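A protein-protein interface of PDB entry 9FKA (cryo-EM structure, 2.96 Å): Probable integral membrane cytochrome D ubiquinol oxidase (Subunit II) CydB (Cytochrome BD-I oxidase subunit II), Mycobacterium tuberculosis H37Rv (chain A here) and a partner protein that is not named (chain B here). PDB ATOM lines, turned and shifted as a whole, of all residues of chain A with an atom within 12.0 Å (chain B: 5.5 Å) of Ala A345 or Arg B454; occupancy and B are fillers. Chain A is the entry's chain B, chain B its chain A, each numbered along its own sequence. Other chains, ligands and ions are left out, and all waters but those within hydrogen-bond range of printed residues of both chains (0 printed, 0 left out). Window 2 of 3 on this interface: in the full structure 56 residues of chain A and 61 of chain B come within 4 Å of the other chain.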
ATOM      1  N   TRP A 107       1.432   2.781  11.001  1.00  0.00           N
ATOM      2  CA  TRP A 107       2.186   2.241  12.123  1.00  0.00           C
ATOM      3  C   TRP A 107       1.313   1.867  13.313  1.00  0.00           C
ATOM      4  O   TRP A 107       1.840   1.360  14.308  1.00  0.00           O
ATOM      5  CB  TRP A 107       3.242   3.250  12.581  1.00  0.00           C
ATOM      6  CG  TRP A 107       4.322   3.503  11.582  1.00  0.00           C
ATOM      7  CD1 TRP A 107       4.446   2.948  10.345  1.00  0.00           C
ATOM      8  CD2 TRP A 107       5.437   4.386  11.737  1.00  0.00           C
ATOM      9  NE1 TRP A 107       5.569   3.429   9.720  1.00  0.00           N
ATOM     10  CE2 TRP A 107       6.195   4.315  10.556  1.00  0.00           C
ATOM     11  CE3 TRP A 107       5.867   5.231  12.764  1.00  0.00           C
ATOM     12  CZ2 TRP A 107       7.358   5.054  10.371  1.00  0.00           C
ATOM     13  CZ3 TRP A 107       7.019   5.964  12.579  1.00  0.00           C
ATOM     14  CH2 TRP A 107       7.753   5.871  11.392  1.00  0.00           C
ATOM     15  N   GLY A 109      -1.005  -0.499  13.859  1.00  0.00           N
ATOM     16  CA  GLY A 109      -1.075  -1.916  14.139  1.00  0.00           C
ATOM     17  C   GLY A 109       0.242  -2.649  14.102  1.00  0.00           C
ATOM     18  O   GLY A 109       0.257  -3.876  14.236  1.00  0.00           O
ATOM     19  N   LYS A 110       1.357  -1.941  13.921  1.00  0.00           N
ATOM     20  CA  LYS A 110       2.648  -2.610  13.825  1.00  0.00           C
ATOM     21  C   LYS A 110       3.118  -3.170  15.160  1.00  0.00           C
ATOM     22  O   LYS A 110       3.986  -4.049  15.172  1.00  0.00           O
ATOM     23  CB  LYS A 110       3.696  -1.647  13.269  1.00  0.00           C
ATOM     24  CG  LYS A 110       3.479  -1.274  11.813  1.00  0.00           C
ATOM     25  CD  LYS A 110       3.812  -2.424  10.877  1.00  0.00           C
ATOM     26  CE  LYS A 110       3.537  -2.050   9.432  1.00  0.00           C
ATOM     27  NZ  LYS A 110       2.079  -1.923   9.162  1.00  0.00           N
ATOM     28  N   ILE A 111       2.576  -2.693  16.278  1.00  0.00           N
ATOM     29  CA  ILE A 111       2.997  -3.135  17.602  1.00  0.00           C
ATOM     30  C   ILE A 111       1.764  -3.294  18.479  1.00  0.00           C
ATOM     31  O   ILE A 111       0.825  -2.496  18.402  1.00  0.00           O
ATOM     32  CB  ILE A 111       4.000  -2.147  18.229  1.00  0.00           C
ATOM     33  CG1 ILE A 111       5.399  -2.406  17.675  1.00  0.00           C
ATOM     34  CG2 ILE A 111       4.022  -2.282  19.741  1.00  0.00           C
ATOM     35  CD1 ILE A 111       6.265  -1.183  17.633  1.00  0.00           C
ATOM     36  N   ASP A 112       1.772  -4.326  19.317  1.00  0.00           N
ATOM     37  CA  ASP A 112       0.664  -4.629  20.221  1.00  0.00           C
ATOM     38  C   ASP A 112       1.047  -4.066  21.586  1.00  0.00           C
ATOM     39  O   ASP A 112       1.714  -4.721  22.387  1.00  0.00           O
ATOM     40  CB  ASP A 112       0.400  -6.135  20.246  1.00  0.00           C
ATOM     41  CG  ASP A 112      -0.331  -6.605  21.498  1.00  0.00           C
ATOM     42  OD1 ASP A 112      -0.725  -5.776  22.340  1.00  0.00           O
ATOM     43  OD2 ASP A 112      -0.538  -7.831  21.629  1.00  0.00           O
ATOM     44  N   ASP A 113       0.611  -2.839  21.850  1.00  0.00           N
ATOM     45  CA  ASP A 113       0.848  -2.203  23.139  1.00  0.00           C
ATOM     46  C   ASP A 113      -0.196  -1.113  23.357  1.00  0.00           C
ATOM     47  O   ASP A 113      -0.343  -0.225  22.507  1.00  0.00           O
ATOM     48  CB  ASP A 113       2.258  -1.615  23.198  1.00  0.00           C
ATOM     49  CG  ASP A 113       2.743  -1.410  24.617  1.00  0.00           C
ATOM     50  OD1 ASP A 113       1.991  -1.737  25.559  1.00  0.00           O
ATOM     51  OD2 ASP A 113       3.879  -0.922  24.794  1.00  0.00           O
ATOM     52  N   TRP A 116       1.268   2.246  22.866  1.00  0.00           N
ATOM     53  CA  TRP A 116       1.611   2.513  21.473  1.00  0.00           C
ATOM     54  C   TRP A 116       0.381   2.928  20.679  1.00  0.00           C
ATOM     55  O   TRP A 116       0.403   3.930  19.955  1.00  0.00           O
ATOM     56  CB  TRP A 116       2.260   1.277  20.849  1.00  0.00           C
ATOM     57  CG  TRP A 116       2.452   1.378  19.367  1.00  0.00           C
ATOM     58  CD1 TRP A 116       1.526   1.114  18.401  1.00  0.00           C
ATOM     59  CD2 TRP A 116       3.647   1.765  18.680  1.00  0.00           C
ATOM     60  NE1 TRP A 116       2.068   1.316  17.156  1.00  0.00           N
ATOM     61  CE2 TRP A 116       3.369   1.715  17.301  1.00  0.00           C
ATOM     62  CE3 TRP A 116       4.922   2.149  19.097  1.00  0.00           C
ATOM     63  CZ2 TRP A 116       4.321   2.035  16.338  1.00  0.00           C
ATOM     64  CZ3 TRP A 116       5.865   2.467  18.140  1.00  0.00           C
ATOM     65  CH2 TRP A 116       5.560   2.407  16.777  1.00  0.00           C
ATOM     66  N   PRO A 338      -5.245  -8.827  15.870  1.00  0.00           N
ATOM     67  CA  PRO A 338      -4.076  -7.959  15.692  1.00  0.00           C
ATOM     68  C   PRO A 338      -2.812  -8.768  15.447  1.00  0.00           C
ATOM     69  O   PRO A 338      -2.614  -9.840  16.022  1.00  0.00           O
ATOM     70  CB  PRO A 338      -4.006  -7.184  17.013  1.00  0.00           C
ATOM     71  CG  PRO A 338      -4.733  -8.032  17.995  1.00  0.00           C
ATOM     72  CD  PRO A 338      -5.815  -8.718  17.223  1.00  0.00           C
ATOM     73  N   THR A 339      -1.950  -8.238  14.580  1.00  0.00           N
ATOM     74  CA  THR A 339      -0.706  -8.894  14.201  1.00  0.00           C
ATOM     75  C   THR A 339       0.524  -8.179  14.746  1.00  0.00           C
ATOM     76  O   THR A 339       1.646  -8.514  14.357  1.00  0.00           O
ATOM     77  CB  THR A 339      -0.609  -8.999  12.678  1.00  0.00           C
ATOM     78  OG1 THR A 339      -0.626  -7.687  12.101  1.00  0.00           O
ATOM     79  CG2 THR A 339      -1.772  -9.808  12.123  1.00  0.00           C
ATOM     80  N   GLY A 340       0.343  -7.204  15.632  1.00  0.00           N
ATOM     81  CA  GLY A 340       1.477  -6.485  16.170  1.00  0.00           C
ATOM     82  C   GLY A 340       2.326  -7.344  17.086  1.00  0.00           C
ATOM     83  O   GLY A 340       1.899  -8.380  17.597  1.00  0.00           O
ATOM     84  N   LEU A 341       3.559  -6.895  17.292  1.00  0.00           N
ATOM     85  CA  LEU A 341       4.515  -7.588  18.141  1.00  0.00           C
ATOM     86  C   LEU A 341       4.565  -6.944  19.521  1.00  0.00           C
ATOM     87  O   LEU A 341       4.312  -5.748  19.679  1.00  0.00           O
ATOM     88  CB  LEU A 341       5.911  -7.573  17.518  1.00  0.00           C
ATOM     89  CG  LEU A 341       5.980  -7.869  16.020  1.00  0.00           C
ATOM     90  CD1 LEU A 341       6.149  -6.595  15.220  1.00  0.00           C
ATOM     91  CD2 LEU A 341       7.112  -8.832  15.729  1.00  0.00           C
ATOM     92  N   ALA A 342       4.897  -7.756  20.522  1.00  0.00           N
ATOM     93  CA  ALA A 342       5.024  -7.247  21.879  1.00  0.00           C
ATOM     94  C   ALA A 342       6.124  -6.197  21.947  1.00  0.00           C
ATOM     95  O   ALA A 342       7.153  -6.305  21.273  1.00  0.00           O
ATOM     96  CB  ALA A 342       5.325  -8.391  22.847  1.00  0.00           C
ATOM     97  N   ARG A 343       5.901  -5.168  22.768  1.00  0.00           N
ATOM     98  CA  ARG A 343       6.885  -4.098  22.887  1.00  0.00           C
ATOM     99  C   ARG A 343       8.215  -4.631  23.404  1.00  0.00           C
ATOM    100  O   ARG A 343       9.281  -4.253  22.905  1.00  0.00           O
ATOM    101  CB  ARG A 343       6.353  -2.997  23.805  1.00  0.00           C
ATOM    102  CG  ARG A 343       7.434  -2.116  24.411  1.00  0.00           C
ATOM    103  CD  ARG A 343       6.885  -0.753  24.804  1.00  0.00           C
ATOM    104  NE  ARG A 343       5.933  -0.844  25.905  1.00  0.00           N
ATOM    105  CZ  ARG A 343       6.163  -0.440  27.149  1.00  0.00           C
ATOM    106  NH1 ARG A 343       7.324   0.086  27.507  1.00  0.00           N
ATOM    107  NH2 ARG A 343       5.203  -0.569  28.060  1.00  0.00           N
ATOM    108  N   ARG A 344       8.174  -5.510  24.403  1.00  0.00           N
ATOM    109  CA  ARG A 344       9.377  -6.125  24.955  1.00  0.00           C
ATOM    110  C   ARG A 344       9.699  -7.369  24.134  1.00  0.00           C
ATOM    111  O   ARG A 344       8.941  -8.344  24.148  1.00  0.00           O
ATOM    112  CB  ARG A 344       9.176  -6.476  26.426  1.00  0.00           C
ATOM    113  CG  ARG A 344       8.994  -5.275  27.340  1.00  0.00           C
ATOM    114  CD  ARG A 344      10.257  -4.430  27.425  1.00  0.00           C
ATOM    115  NE  ARG A 344      10.114  -3.161  26.722  1.00  0.00           N
ATOM    116  CZ  ARG A 344      11.129  -2.414  26.307  1.00  0.00           C
ATOM    117  NH1 ARG A 344      12.384  -2.775  26.513  1.00  0.00           N
ATOM    118  NH2 ARG A 344      10.876  -1.274  25.669  1.00  0.00           N
ATOM    119  N   ALA A 345      10.816  -7.336  23.421  1.00  0.00           N
ATOM    120  CA  ALA A 345      11.205  -8.476  22.601  1.00  0.00           C
ATOM    121  C   ALA A 345      11.507  -9.673  23.498  1.00  0.00           C
ATOM    122  O   ALA A 345      12.280  -9.542  24.455  1.00  0.00           O
ATOM    123  CB  ALA A 345      12.424  -8.132  21.752  1.00  0.00           C
ATOM    124  N   PRO A 346      10.914 -10.878  23.280  1.00  0.00           N
ATOM    125  CA  PRO A 346      11.123 -12.032  24.208  1.00  0.00           C
ATOM    126  C   PRO A 346      12.612 -12.322  24.364  1.00  0.00           C
ATOM    127  O   PRO A 346      13.282 -12.503  23.347  1.00  0.00           O
ATOM    128  CB  PRO A 346      10.364 -13.188  23.560  1.00  0.00           C
ATOM    129  CG  PRO A 346       9.298 -12.490  22.740  1.00  0.00           C
ATOM    130  CD  PRO A 346       9.993 -11.302  22.165  1.00  0.00           C
ATOM    131  OXT PRO A 346      13.077 -12.361  25.519  1.00  0.00           O
ATOM    132  N   CYS B 449      13.396   3.788  12.833  1.00  0.00           N
ATOM    133  CA  CYS B 449      14.543   2.909  13.023  1.00  0.00           C
ATOM    134  C   CYS B 449      14.220   1.799  14.014  1.00  0.00           C
ATOM    135  O   CYS B 449      14.574   0.634  13.792  1.00  0.00           O
ATOM    136  CB  CYS B 449      15.750   3.716  13.497  1.00  0.00           C
ATOM    137  SG  CYS B 449      17.231   2.727  13.785  1.00  0.00           S
ATOM    138  N   TRP B 450      13.543   2.138  15.112  1.00  0.00           N
ATOM    139  CA  TRP B 450      13.202   1.120  16.099  1.00  0.00           C
ATOM    140  C   TRP B 450      12.246   0.087  15.518  1.00  0.00           C
ATOM    141  O   TRP B 450      12.386  -1.114  15.778  1.00  0.00           O
ATOM    142  CB  TRP B 450      12.593   1.772  17.337  1.00  0.00           C
ATOM    143  CG  TRP B 450      12.432   0.821  18.472  1.00  0.00           C
ATOM    144  CD1 TRP B 450      13.424   0.270  19.226  1.00  0.00           C
ATOM    145  CD2 TRP B 450      11.203   0.300  18.983  1.00  0.00           C
ATOM    146  NE1 TRP B 450      12.890  -0.561  20.178  1.00  0.00           N
ATOM    147  CE2 TRP B 450      11.526  -0.560  20.050  1.00  0.00           C
ATOM    148  CE3 TRP B 450       9.860   0.477  18.644  1.00  0.00           C
ATOM    149  CZ2 TRP B 450      10.557  -1.240  20.778  1.00  0.00           C
ATOM    150  CZ3 TRP B 450       8.901  -0.197  19.369  1.00  0.00           C
ATOM    151  CH2 TRP B 450       9.252  -1.046  20.423  1.00  0.00           C
ATOM    152  N   LEU B 451      11.258   0.532  14.739  1.00  0.00           N
ATOM    153  CA  LEU B 451      10.327  -0.402  14.116  1.00  0.00           C
ATOM    154  C   LEU B 451      11.045  -1.325  13.144  1.00  0.00           C
ATOM    155  O   LEU B 451      10.779  -2.533  13.107  1.00  0.00           O
ATOM    156  CB  LEU B 451       9.219   0.365  13.394  1.00  0.00           C
ATOM    157  CG  LEU B 451       7.918   0.553  14.171  1.00  0.00           C
ATOM    158  CD1 LEU B 451       7.078   1.644  13.537  1.00  0.00           C
ATOM    159  CD2 LEU B 451       7.143  -0.748  14.231  1.00  0.00           C
ATOM    160  N   LEU B 452      11.955  -0.772  12.338  1.00  0.00           N
ATOM    161  CA  LEU B 452      12.712  -1.612  11.419  1.00  0.00           C
ATOM    162  C   LEU B 452      13.537  -2.638  12.180  1.00  0.00           C
ATOM    163  O   LEU B 452      13.594  -3.808  11.791  1.00  0.00           O
ATOM    164  CB  LEU B 452      13.613  -0.752  10.533  1.00  0.00           C
ATOM    165  CG  LEU B 452      12.956  -0.019   9.362  1.00  0.00           C
ATOM    166  CD1 LEU B 452      14.019   0.629   8.499  1.00  0.00           C
ATOM    167  CD2 LEU B 452      12.098  -0.950   8.524  1.00  0.00           C
ATOM    168  N   LYS B 453      14.177  -2.222  13.274  1.00  0.00           N
ATOM    169  CA  LYS B 453      14.941  -3.170  14.079  1.00  0.00           C
ATOM    170  C   LYS B 453      14.040  -4.274  14.618  1.00  0.00           C
ATOM    171  O   LYS B 453      14.370  -5.465  14.527  1.00  0.00           O
ATOM    172  CB  LYS B 453      15.636  -2.440  15.228  1.00  0.00           C
ATOM    173  CG  LYS B 453      15.927  -3.323  16.431  1.00  0.00           C
ATOM    174  CD  LYS B 453      16.911  -2.669  17.383  1.00  0.00           C
ATOM    175  CE  LYS B 453      17.383  -3.648  18.444  1.00  0.00           C
ATOM    176  NZ  LYS B 453      16.251  -4.198  19.238  1.00  0.00           N
ATOM    177  N   ARG B 454      12.887  -3.897  15.172  1.00  0.00           N
ATOM    178  CA  ARG B 454      11.998  -4.882  15.775  1.00  0.00           C
ATOM    179  C   ARG B 454      11.505  -5.881  14.740  1.00  0.00           C
ATOM    180  O   ARG B 454      11.430  -7.084  15.014  1.00  0.00           O
ATOM    181  CB  ARG B 454      10.815  -4.186  16.446  1.00  0.00           C
ATOM    182  CG  ARG B 454      11.125  -3.621  17.822  1.00  0.00           C
ATOM    183  CD  ARG B 454      11.236  -4.717  18.871  1.00  0.00           C
ATOM    184  NE  ARG B 454       9.964  -5.400  19.083  1.00  0.00           N
ATOM    185  CZ  ARG B 454       9.787  -6.716  19.044  1.00  0.00           C
ATOM    186  NH1 ARG B 454      10.790  -7.547  18.807  1.00  0.00           N
ATOM    187  NH2 ARG B 454       8.571  -7.211  19.251  1.00  0.00           N
ATOM    188  N   TYR B 455      11.157  -5.405  13.546  1.00  0.00           N
ATOM    189  CA  TYR B 455      10.651  -6.314  12.524  1.00  0.00           C
ATOM    190  C   TYR B 455      11.761  -7.153  11.906  1.00  0.00           C
ATOM    191  O   TYR B 455      11.506  -8.285  11.481  1.00  0.00           O
ATOM    192  CB  TYR B 455       9.912  -5.530  11.442  1.00  0.00           C
ATOM    193  CG  TYR B 455       8.434  -5.406  11.720  1.00  0.00           C
ATOM    194  CD1 TYR B 455       7.947  -4.416  12.558  1.00  0.00           C
ATOM    195  CD2 TYR B 455       7.526  -6.287  11.154  1.00  0.00           C
ATOM    196  CE1 TYR B 455       6.600  -4.303  12.820  1.00  0.00           C
ATOM    197  CE2 TYR B 455       6.177  -6.181  11.410  1.00  0.00           C
ATOM    198  CZ  TYR B 455       5.718  -5.187  12.244  1.00  0.00           C
ATOM    199  OH  TYR B 455       4.373  -5.078  12.503  1.00  0.00           O
ATOM    200  N   ILE B 456      12.986  -6.630  11.845  1.00  0.00           N
ATOM    201  CA  ILE B 456      14.093  -7.412  11.309  1.00  0.00           C
ATOM    202  C   ILE B 456      14.471  -8.531  12.270  1.00  0.00           C
ATOM    203  O   ILE B 456      14.754  -9.657  11.848  1.00  0.00           O
ATOM    204  CB  ILE B 456      15.290  -6.495  11.003  1.00  0.00           C
ATOM    205  CG1 ILE B 456      15.013  -5.667   9.748  1.00  0.00           C
ATOM    206  CG2 ILE B 456      16.555  -7.312  10.822  1.00  0.00           C
ATOM    207  CD1 ILE B 456      15.861  -4.421   9.637  1.00  0.00           C
ATOM    208  N   VAL B 457      14.486  -8.246  13.575  1.00  0.00           N
ATOM    209  CA  VAL B 457      14.865  -9.267  14.547  1.00  0.00           C
ATOM    210  C   VAL B 457      13.859 -10.402  14.629  1.00  0.00           C
ATOM    211  O   VAL B 457      14.169 -11.448  15.210  1.00  0.00           O
ATOM    212  CB  VAL B 457      15.059  -8.655  15.950  1.00  0.00           C
ATOM    213  CG1 VAL B 457      16.193  -7.642  15.935  1.00  0.00           C
ATOM    214  CG2 VAL B 457      13.772  -8.015  16.446  1.00  0.00           C
ATOM    215  N   GLU B 458      12.663 -10.225  14.072  1.00  0.00           N
ATOM    216  CA  GLU B 458      11.647 -11.269  14.070  1.00  0.00           C
ATOM    217  C   GLU B 458      11.666 -12.122  12.814  1.00  0.00           C
ATOM    218  O   GLU B 458      11.315 -13.304  12.877  1.00  0.00           O
ATOM    219  CB  GLU B 458      10.252 -10.648  14.222  1.00  0.00           C
ATOM    220  CG  GLU B 458       9.225 -11.514  14.954  1.00  0.00           C
ATOM    221  CD  GLU B 458       9.612 -11.877  16.385  1.00  0.00           C
ATOM    222  OE1 GLU B 458      10.806 -11.810  16.737  1.00  0.00           O
ATOM    223  OE2 GLU B 458       8.707 -12.235  17.166  1.00  0.00           O
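O of Ala A342 lies within hydrogen-bond range of NH2 of Arg B454 (2.6 Å). OH of Tyr B455 lies within hydrogen-bond range of O of Lys A110, at 2.9 Å.
NE1 of Trp A116 lies within hydrogen-bond range of O of Trp A107 (2.9 Å). The backbone NH (N) of Asp A112 lies within hydrogen-bond range of the backbone carbonyl oxygen (O) of Leu A341 (2.9 Å). The side-chain carboxylate (OD2) of Asp A113 lies within salt-bridge range of the guanidinium group (NH2) of Arg A343.
Among the printed residues, pairs that only touch across the chains: Leu A341 with Arg B454 (3.2 Å), Ile A111 with Trp B450 (3.3 Å), Leu A341 with Tyr B455 (3.3 Å), Ala A345 with Arg B454 (3.4 Å), Leu A341 with Glu B458 (3.5 Å), Ile A111 with Leu B451 (3.5 Å), Trp A116 with Leu B451 (3.7 Å), Trp A107 with Leu B451 (3.7 Å), Lys A110 with Leu B451 (3.7 Å) and Arg A343 with Trp B450 (3.9 Å).
Of the printed residues of chain B, Ala A345 touches Arg B454. Of chain A, only Leu A341 (3.2 Å), Ala A342 (2.6 Å) and Ala A345 (3.4 Å) come within 4 Å of Arg B454. Trp B450 touches just these residues of chain A: Ile A111 and Arg A343. Leu B451 touches just these residues of chain A: Trp A107, Lys A110, Ile A111 and Trp A116. No residue of chain A comes within 4 Å of Lys B453. Of chain A, only Lys A110 (2.9 Å) and Leu A341 (3.3 Å) come within 4 Å of Tyr B455. No residue of chain A comes within 4 Å of Ile B456. No residue of chain A comes within 4 Å of Val B457. Of the printed residues of chain B, Ala A342 touches Arg B454 (2.6 Å). Printed residues of chain B within 4 Å of Leu A341: Arg B454 (3.2 Å), Tyr B455 (3.3 Å) and Glu B458 (3.5 Å). Of the printed residues of chain B, Trp A107 touches Leu B451. Printed residues of chain B within 4 Å of Arg A343: Trp B450. Printed residues of chain B within 4 Å of Trp A116: Leu B451. Pro A338 touches none of the printed residues of chain B. Asp A112 touches none of the printed residues of chain B.
Of the 16 printed residues of chain A, 8 touch a printed residue of chain B. Hydrophobic or aromatic side chains of chain A within 4 Å of the printed part of chain B: Trp A107, Ile A111, Trp A116, Leu A341 and Ala A345. Along chain A the printed residues that touch a printed residue of chain B span positions 107 to 345. Hydrophobic or aromatic side chains of chain B that line the printed part of chain A: Trp B450, Leu B451 and Tyr B455. Among the printed residues, 12 pairs touch across the chains. Among the printed residues, no Asp or Glu carboxylate lies within 4 Å of a Lys or Arg side-chain nitrogen of the other chain.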
